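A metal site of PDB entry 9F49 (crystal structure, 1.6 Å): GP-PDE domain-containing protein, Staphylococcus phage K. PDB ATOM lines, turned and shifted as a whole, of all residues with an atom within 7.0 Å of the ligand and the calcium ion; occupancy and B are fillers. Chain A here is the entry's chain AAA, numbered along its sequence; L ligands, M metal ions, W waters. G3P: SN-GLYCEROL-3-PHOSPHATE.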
ATOM      1  N   HIS A   8       2.320  -3.902  19.442  1.00  0.00           N
ATOM      2  CA  HIS A   8       1.870  -3.449  20.785  1.00  0.00           C
ATOM      3  C   HIS A   8       2.134  -4.561  21.797  1.00  0.00           C
ATOM      4  O   HIS A   8       1.503  -5.610  21.704  1.00  0.00           O
ATOM      5  CB  HIS A   8       0.389  -3.068  20.724  1.00  0.00           C
ATOM      6  CG  HIS A   8      -0.156  -2.496  21.988  1.00  0.00           C
ATOM      7  ND1 HIS A   8      -1.152  -3.140  22.690  1.00  0.00           N
ATOM      8  CD2 HIS A   8       0.118  -1.360  22.663  1.00  0.00           C
ATOM      9  CE1 HIS A   8      -1.476  -2.413  23.750  1.00  0.00           C
ATOM     10  NE2 HIS A   8      -0.707  -1.315  23.752  1.00  0.00           N
ATOM     11  N   ARG A   9       3.034  -4.298  22.756  1.00  0.00           N
ATOM     12  CA  ARG A   9       3.503  -5.257  23.783  1.00  0.00           C
ATOM     13  C   ARG A   9       3.962  -6.560  23.116  1.00  0.00           C
ATOM     14  O   ARG A   9       3.882  -7.617  23.765  1.00  0.00           O
ATOM     15  CB  ARG A   9       2.403  -5.494  24.821  1.00  0.00           C
ATOM     16  CG  ARG A   9       1.703  -4.226  25.281  1.00  0.00           C
ATOM     17  CD  ARG A   9       0.730  -4.409  26.427  1.00  0.00           C
ATOM     18  NE  ARG A   9      -0.095  -3.229  26.601  1.00  0.00           N
ATOM     19  CZ  ARG A   9      -1.236  -3.178  27.294  1.00  0.00           C
ATOM     20  NH1 ARG A   9      -1.688  -4.247  27.924  1.00  0.00           N
ATOM     21  NH2 ARG A   9      -1.934  -2.057  27.322  1.00  0.00           N
ATOM     22  N   HIS A  18       4.362  -8.816  26.337  1.00  0.00           N
ATOM     23  CA  HIS A  18       5.665  -8.572  27.013  1.00  0.00           C
ATOM     24  C   HIS A  18       6.331  -9.887  27.384  1.00  0.00           C
ATOM     25  O   HIS A  18       6.719 -10.060  28.547  1.00  0.00           O
ATOM     26  CB  HIS A  18       5.483  -7.656  28.224  1.00  0.00           C
ATOM     27  CG  HIS A  18       5.053  -6.296  27.815  1.00  0.00           C
ATOM     28  ND1 HIS A  18       5.647  -5.634  26.761  1.00  0.00           N
ATOM     29  CD2 HIS A  18       4.130  -5.462  28.332  1.00  0.00           C
ATOM     30  CE1 HIS A  18       5.088  -4.449  26.625  1.00  0.00           C
ATOM     31  NE2 HIS A  18       4.164  -4.318  27.577  1.00  0.00           N
ATOM     32  N   GLU A  35       7.295  -3.168  20.858  1.00  0.00           N
ATOM     33  CA  GLU A  35       6.944  -2.137  21.864  1.00  0.00           C
ATOM     34  C   GLU A  35       7.083  -2.716  23.274  1.00  0.00           C
ATOM     35  O   GLU A  35       6.422  -3.724  23.577  1.00  0.00           O
ATOM     36  CB  GLU A  35       5.529  -1.624  21.617  1.00  0.00           C
ATOM     37  CG  GLU A  35       5.235  -0.391  22.448  1.00  0.00           C
ATOM     38  CD  GLU A  35       4.035  -0.445  23.373  1.00  0.00           C
ATOM     39  OE1 GLU A  35       3.338  -1.472  23.422  1.00  0.00           O
ATOM     40  OE2 GLU A  35       3.798   0.590  24.051  1.00  0.00           O
ATOM     41  N   LEU A  36       7.933  -2.098  24.089  1.00  0.00           N
ATOM     42  CA  LEU A  36       8.155  -2.444  25.513  1.00  0.00           C
ATOM     43  C   LEU A  36       7.476  -1.366  26.369  1.00  0.00           C
ATOM     44  O   LEU A  36       7.639  -0.175  26.044  1.00  0.00           O
ATOM     45  CB  LEU A  36       9.653  -2.475  25.818  1.00  0.00           C
ATOM     46  CG  LEU A  36      10.443  -3.682  25.321  1.00  0.00           C
ATOM     47  CD1 LEU A  36      10.317  -3.868  23.825  1.00  0.00           C
ATOM     48  CD2 LEU A  36      11.907  -3.550  25.731  1.00  0.00           C
ATOM     49  N   ASP A  37       6.771  -1.779  27.421  1.00  0.00           N
ATOM     50  CA  ASP A  37       6.386  -0.914  28.567  1.00  0.00           C
ATOM     51  C   ASP A  37       7.315  -1.317  29.706  1.00  0.00           C
ATOM     52  O   ASP A  37       7.501  -2.525  29.886  1.00  0.00           O
ATOM     53  CB  ASP A  37       4.942  -1.129  29.005  1.00  0.00           C
ATOM     54  CG  ASP A  37       3.902  -0.840  27.932  1.00  0.00           C
ATOM     55  OD1 ASP A  37       3.938   0.251  27.359  1.00  0.00           O
ATOM     56  OD2 ASP A  37       3.067  -1.738  27.679  1.00  0.00           O
ATOM     57  N   HIS A  50       3.233  -3.837  31.604  1.00  0.00           N
ATOM     58  CA  HIS A  50       2.347  -2.676  31.337  1.00  0.00           C
ATOM     59  C   HIS A  50       1.857  -2.081  32.663  1.00  0.00           C
ATOM     60  O   HIS A  50       2.049  -0.855  32.885  1.00  0.00           O
ATOM     61  CB  HIS A  50       1.191  -3.076  30.432  1.00  0.00           C
ATOM     62  CG  HIS A  50       0.224  -1.960  30.311  1.00  0.00           C
ATOM     63  ND1 HIS A  50      -0.824  -1.802  31.198  1.00  0.00           N
ATOM     64  CD2 HIS A  50       0.194  -0.908  29.478  1.00  0.00           C
ATOM     65  CE1 HIS A  50      -1.489  -0.707  30.881  1.00  0.00           C
ATOM     66  NE2 HIS A  50      -0.890  -0.141  29.827  1.00  0.00           N
ATOM     67  N   TYR A 101      10.548   0.351  20.506  1.00  0.00           N
ATOM     68  CA  TYR A 101       9.649   1.484  20.839  1.00  0.00           C
ATOM     69  C   TYR A 101       9.326   1.331  22.327  1.00  0.00           C
ATOM     70  O   TYR A 101       8.598   0.404  22.692  1.00  0.00           O
ATOM     71  CB  TYR A 101       8.430   1.461  19.904  1.00  0.00           C
ATOM     72  CG  TYR A 101       7.810   2.808  19.628  1.00  0.00           C
ATOM     73  CD1 TYR A 101       7.239   3.540  20.640  1.00  0.00           C
ATOM     74  CD2 TYR A 101       7.762   3.335  18.352  1.00  0.00           C
ATOM     75  CE1 TYR A 101       6.647   4.765  20.418  1.00  0.00           C
ATOM     76  CE2 TYR A 101       7.180   4.569  18.102  1.00  0.00           C
ATOM     77  CZ  TYR A 101       6.621   5.303  19.142  1.00  0.00           C
ATOM     78  OH  TYR A 101       6.017   6.515  18.922  1.00  0.00           O
ATOM     79  N   GLU A 103       8.376   2.525  26.251  1.00  0.00           N
ATOM     80  CA  GLU A 103       7.625   3.441  27.135  1.00  0.00           C
ATOM     81  C   GLU A 103       8.168   3.395  28.564  1.00  0.00           C
ATOM     82  O   GLU A 103       8.261   2.303  29.158  1.00  0.00           O
ATOM     83  CB  GLU A 103       6.138   3.105  27.124  1.00  0.00           C
ATOM     84  CG  GLU A 103       5.314   4.100  27.923  1.00  0.00           C
ATOM     85  CD  GLU A 103       3.809   3.920  27.795  1.00  0.00           C
ATOM     86  OE1 GLU A 103       3.383   3.117  26.933  1.00  0.00           O
ATOM     87  OE2 GLU A 103       3.066   4.566  28.572  1.00  0.00           O
ATOM     88  N   LYS A 105       6.831   3.977  31.999  1.00  0.00           N
ATOM     89  CA  LYS A 105       5.503   4.042  32.657  1.00  0.00           C
ATOM     90  C   LYS A 105       5.595   4.992  33.839  1.00  0.00           C
ATOM     91  O   LYS A 105       6.699   5.241  34.349  1.00  0.00           O
ATOM     92  CB  LYS A 105       5.033   2.632  33.045  1.00  0.00           C
ATOM     93  CG  LYS A 105       4.449   1.830  31.884  1.00  0.00           C
ATOM     94  CD  LYS A 105       3.181   2.477  31.334  1.00  0.00           C
ATOM     95  CE  LYS A 105       2.528   1.725  30.201  1.00  0.00           C
ATOM     96  NZ  LYS A 105       1.429   2.523  29.607  1.00  0.00           N
ATOM     97  N   GLN A 138       8.970   6.671  24.324  1.00  0.00           N
ATOM     98  CA  GLN A 138       7.612   7.250  24.444  1.00  0.00           C
ATOM     99  C   GLN A 138       7.242   7.340  25.927  1.00  0.00           C
ATOM    100  O   GLN A 138       7.739   6.526  26.725  1.00  0.00           O
ATOM    101  CB  GLN A 138       6.569   6.408  23.695  1.00  0.00           C
ATOM    102  CG  GLN A 138       6.702   4.923  23.991  1.00  0.00           C
ATOM    103  CD  GLN A 138       5.537   4.050  23.590  1.00  0.00           C
ATOM    104  OE1 GLN A 138       4.480   4.514  23.201  1.00  0.00           O
ATOM    105  NE2 GLN A 138       5.731   2.741  23.725  1.00  0.00           N
ATOM    106  N   SER A 139       6.421   8.310  26.282  1.00  0.00           N
ATOM    107  CA  SER A 139       5.877   8.409  27.653  1.00  0.00           C
ATOM    108  C   SER A 139       4.650   9.322  27.683  1.00  0.00           C
ATOM    109  O   SER A 139       4.541  10.226  26.837  1.00  0.00           O
ATOM    110  CB  SER A 139       6.930   8.896  28.601  1.00  0.00           C
ATOM    111  OG  SER A 139       6.533   8.703  29.949  1.00  0.00           O
ATOM    112  N   PHE A 140       3.749   9.056  28.622  1.00  0.00           N
ATOM    113  CA  PHE A 140       2.700  10.016  29.064  1.00  0.00           C
ATOM    114  C   PHE A 140       3.322  11.073  29.984  1.00  0.00           C
ATOM    115  O   PHE A 140       2.712  12.138  30.155  1.00  0.00           O
ATOM    116  CB  PHE A 140       1.581   9.288  29.805  1.00  0.00           C
ATOM    117  CG  PHE A 140       0.611   8.542  28.913  1.00  0.00           C
ATOM    118  CD1 PHE A 140       0.816   7.216  28.611  1.00  0.00           C
ATOM    119  CD2 PHE A 140      -0.515   9.171  28.405  1.00  0.00           C
ATOM    120  CE1 PHE A 140      -0.087   6.524  27.818  1.00  0.00           C
ATOM    121  CE2 PHE A 140      -1.403   8.485  27.597  1.00  0.00           C
ATOM    122  CZ  PHE A 140      -1.203   7.153  27.312  1.00  0.00           C
ATOM    123  N   LEU A 160       2.932  10.581  24.456  1.00  0.00           N
ATOM    124  CA  LEU A 160       1.682   9.792  24.471  1.00  0.00           C
ATOM    125  C   LEU A 160       0.554  10.670  25.013  1.00  0.00           C
ATOM    126  O   LEU A 160       0.755  11.343  26.064  1.00  0.00           O
ATOM    127  CB  LEU A 160       1.859   8.536  25.335  1.00  0.00           C
ATOM    128  CG  LEU A 160       2.691   7.445  24.693  1.00  0.00           C
ATOM    129  CD1 LEU A 160       3.177   6.444  25.721  1.00  0.00           C
ATOM    130  CD2 LEU A 160       1.896   6.740  23.586  1.00  0.00           C
ATOM    131  N   ALA A 181       1.824  10.838  19.841  1.00  0.00           N
ATOM    132  CA  ALA A 181       1.277   9.474  19.783  1.00  0.00           C
ATOM    133  C   ALA A 181      -0.094   9.506  20.437  1.00  0.00           C
ATOM    134  O   ALA A 181      -0.216   9.272  21.639  1.00  0.00           O
ATOM    135  CB  ALA A 181       2.231   8.520  20.439  1.00  0.00           C
ATOM    136  N   HIS A 203       1.839   8.849  15.568  1.00  0.00           N
ATOM    137  CA  HIS A 203       1.816   7.380  15.794  1.00  0.00           C
ATOM    138  C   HIS A 203       0.580   7.042  16.616  1.00  0.00           C
ATOM    139  O   HIS A 203       0.558   7.358  17.807  1.00  0.00           O
ATOM    140  CB  HIS A 203       3.103   6.928  16.489  1.00  0.00           C
ATOM    141  CG  HIS A 203       4.339   7.203  15.724  1.00  0.00           C
ATOM    142  ND1 HIS A 203       5.581   7.228  16.320  1.00  0.00           N
ATOM    143  CD2 HIS A 203       4.550   7.439  14.406  1.00  0.00           C
ATOM    144  CE1 HIS A 203       6.501   7.492  15.421  1.00  0.00           C
ATOM    145  NE2 HIS A 203       5.890   7.624  14.224  1.00  0.00           N
ATOM    146  N   ALA A 204      -0.414   6.436  15.991  1.00  0.00           N
ATOM    147  CA  ALA A 204      -1.750   6.205  16.583  1.00  0.00           C
ATOM    148  C   ALA A 204      -1.784   4.871  17.335  1.00  0.00           C
ATOM    149  O   ALA A 204      -1.196   3.901  16.856  1.00  0.00           O
ATOM    150  CB  ALA A 204      -2.776   6.219  15.481  1.00  0.00           C
ATOM    151  N   TRP A 205      -2.484   4.820  18.476  1.00  0.00           N
ATOM    152  CA  TRP A 205      -2.628   3.585  19.294  1.00  0.00           C
ATOM    153  C   TRP A 205      -4.052   3.477  19.823  1.00  0.00           C
ATOM    154  O   TRP A 205      -4.705   4.499  20.020  1.00  0.00           O
ATOM    155  CB  TRP A 205      -1.655   3.625  20.476  1.00  0.00           C
ATOM    156  CG  TRP A 205      -1.831   4.826  21.358  1.00  0.00           C
ATOM    157  CD1 TRP A 205      -1.181   6.028  21.257  1.00  0.00           C
ATOM    158  CD2 TRP A 205      -2.682   4.944  22.509  1.00  0.00           C
ATOM    159  NE1 TRP A 205      -1.590   6.873  22.242  1.00  0.00           N
ATOM    160  CE2 TRP A 205      -2.507   6.244  23.032  1.00  0.00           C
ATOM    161  CE3 TRP A 205      -3.578   4.071  23.150  1.00  0.00           C
ATOM    162  CZ2 TRP A 205      -3.194   6.687  24.156  1.00  0.00           C
ATOM    163  CZ3 TRP A 205      -4.269   4.531  24.257  1.00  0.00           C
ATOM    164  CH2 TRP A 205      -4.074   5.822  24.749  1.00  0.00           C
ATOM    165  N   THR A 206      -4.547   2.265  20.129  1.00  0.00           N
ATOM    166  CA  THR A 206      -4.061   0.983  19.647  1.00  0.00           C
ATOM    167  C   THR A 206      -5.134   0.447  18.686  1.00  0.00           C
ATOM    168  O   THR A 206      -6.260   0.209  19.145  1.00  0.00           O
ATOM    169  CB  THR A 206      -3.813   0.000  20.802  1.00  0.00           C
ATOM    170  OG1 THR A 206      -2.771   0.529  21.627  1.00  0.00           O
ATOM    171  CG2 THR A 206      -3.442  -1.386  20.332  1.00  0.00           C
ATOM    172  N   PHE A 225       0.275   1.453  16.460  1.00  0.00           N
ATOM    173  CA  PHE A 225       0.447   0.300  17.360  1.00  0.00           C
ATOM    174  C   PHE A 225      -0.775  -0.596  17.200  1.00  0.00           C
ATOM    175  O   PHE A 225      -1.899  -0.080  17.198  1.00  0.00           O
ATOM    176  CB  PHE A 225       0.527   0.762  18.818  1.00  0.00           C
ATOM    177  CG  PHE A 225       1.578   1.772  19.174  1.00  0.00           C
ATOM    178  CD1 PHE A 225       1.440   3.104  18.798  1.00  0.00           C
ATOM    179  CD2 PHE A 225       2.628   1.429  20.007  1.00  0.00           C
ATOM    180  CE1 PHE A 225       2.384   4.046  19.182  1.00  0.00           C
ATOM    181  CE2 PHE A 225       3.571   2.381  20.394  1.00  0.00           C
ATOM    182  CZ  PHE A 225       3.435   3.686  19.975  1.00  0.00           C
HETATM  183  O1  G3P L   1       2.307   3.271  23.989  1.00  0.00           O
HETATM  184  C1  G3P L   1       1.169   3.286  23.140  1.00  0.00           C
HETATM  185  C2  G3P L   1       0.012   2.690  23.894  1.00  0.00           C
HETATM  186  O2  G3P L   1       0.400   1.367  24.279  1.00  0.00           O
HETATM  187  C3  G3P L   1      -0.326   3.509  25.117  1.00  0.00           C
HETATM  188  O1P G3P L   1      -1.307   2.867  25.936  1.00  0.00           O
HETATM  189  O4P G3P L   1      -1.828   1.709  28.029  1.00  0.00           O
HETATM  190  O2P G3P L   1      -1.353   0.340  25.970  1.00  0.00           O
HETATM  191  O3P G3P L   1       0.552   1.572  27.154  1.00  0.00           O
HETATM  192  P   G3P L   1      -0.946   1.544  26.804  1.00  0.00           P
HETATM  193 CA    CA M   1       2.447   1.364  25.742  1.00  0.00          CA
HETATM  194  O   HOH W   1      -3.535   0.393  24.346  1.00  0.00           O
HETATM  195  O   HOH W   2      -3.000   3.954  28.932  1.00  0.00           O
HETATM  196  O   HOH W   3      -4.214   0.253  28.120  1.00  0.00           O
HETATM  197  O   HOH W   4       1.742  -0.946  25.576  1.00  0.00           O
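Water W4 lies within hydrogen-bond range of the side-chain carboxylate of Asp 37 (2.6 Å), the side-chain carboxylate of Glu 35 (2.7 Å), a ring nitrogen (NE2) of His 8 (3.1 Å), the guanidinium group of Arg 9 (3.1 Å) and an oxygen (O2P) of the ligand (3.4 Å).
Water W1 lies within hydrogen-bond range of an oxygen (O2P) of the ligand (2.7 Å), the side-chain hydroxyl (OG1) of Thr 206 (2.8 Å) and a ring nitrogen (NE2) of His 8 (3.4 Å).
Water W3 bridges an oxygen (O4P) of the ligand (2.8 Å) and the guanidinium group of Arg 9 (3.3 Å).
The guanidinium group (NE) of Arg 9 lies within salt-bridge range of the side-chain carboxylate (OD2) of Asp 37, 3.7 Å away.
The side-chain amide nitrogen of Gln 138 sits close to the side-chain carboxylate of Glu 35.
The backbone carbonyl oxygen (O) of Ala 181 is in hydrogen-bond range of the indole nitrogen (NE1) of Trp 205 (2.8 Å).
The backbone NH of Leu 160 lies within hydrogen-bond range of the backbone carbonyl oxygen of Ser 139, 2.9 Å away.
O of Ala 204 sits at hydrogen-bond distance from N of Phe 225 (2.9 Å).
The guanidinium group (NE) of Arg 9 sits close to a ring nitrogen (NE2) of His 8, 3.5 Å away.
The backbone carbonyl oxygen (O) of Arg 9 sits at hydrogen-bond distance from the backbone NH (N) of His 18.
NE2 of His 50 sits close to NH2 of Arg 9 (3.3 Å).
An oxygen (O4P) of the ligand lies within hydrogen-bond range of a ring nitrogen (NE2) of His 50 (2.7 Å).
An oxygen (O2P) of the ligand lies within hydrogen-bond range of a ring nitrogen (NE2) of His 8 (2.8 Å).
The guanidinium group (NH2) of Arg 9 is in salt-bridge range of an oxygen (O2P) of the ligand, 2.8 Å away.
NZ of Lys 105 lies within salt-bridge range of O4P of the ligand, at 3.7 Å.
The side-chain amide oxygen of Gln 138 sits close to an oxygen (O1) of the ligand (2.6 Å).
Of the 20 residues printed, 3 come within 4 Å of the calcium ion.
The calcium ion is bound by OE2 of Glu 35, at 2.3 Å.
OE1 of Glu 103 is bound to the calcium ion (2.3 Å).
O3P of the ligand is bound to the calcium ion.
Water W4 is bound to the calcium ion.
The calcium ion is bound by OD1 of Asp 37.
O2 of the ligand binds the calcium ion, at 2.5 Å.
O1 of the ligand is bound to the calcium ion (2.6 Å).
Leu 160 touches the ligand (CD2 to O1, 3.5 Å).
Trp 205 touches the ligand (CD2 to C2, 3.8 Å).
CE2 of Phe 225 touches C1 of the ligand, at 3.8 Å.
Hydrophobic or aromatic side chains that line the ligand: His 8, His 50, Leu 160, Trp 205 and Phe 225.
11 residues have an atom within 4 Å of the ligand: His 8, Arg 9, Glu 35, Asp 37, His 50, Glu 103, Lys 105, Gln 138, Leu 160, Trp 205 and Phe 225.
The nearest printed residue that does not touch the ligand is Phe 140 (4.1 Å).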
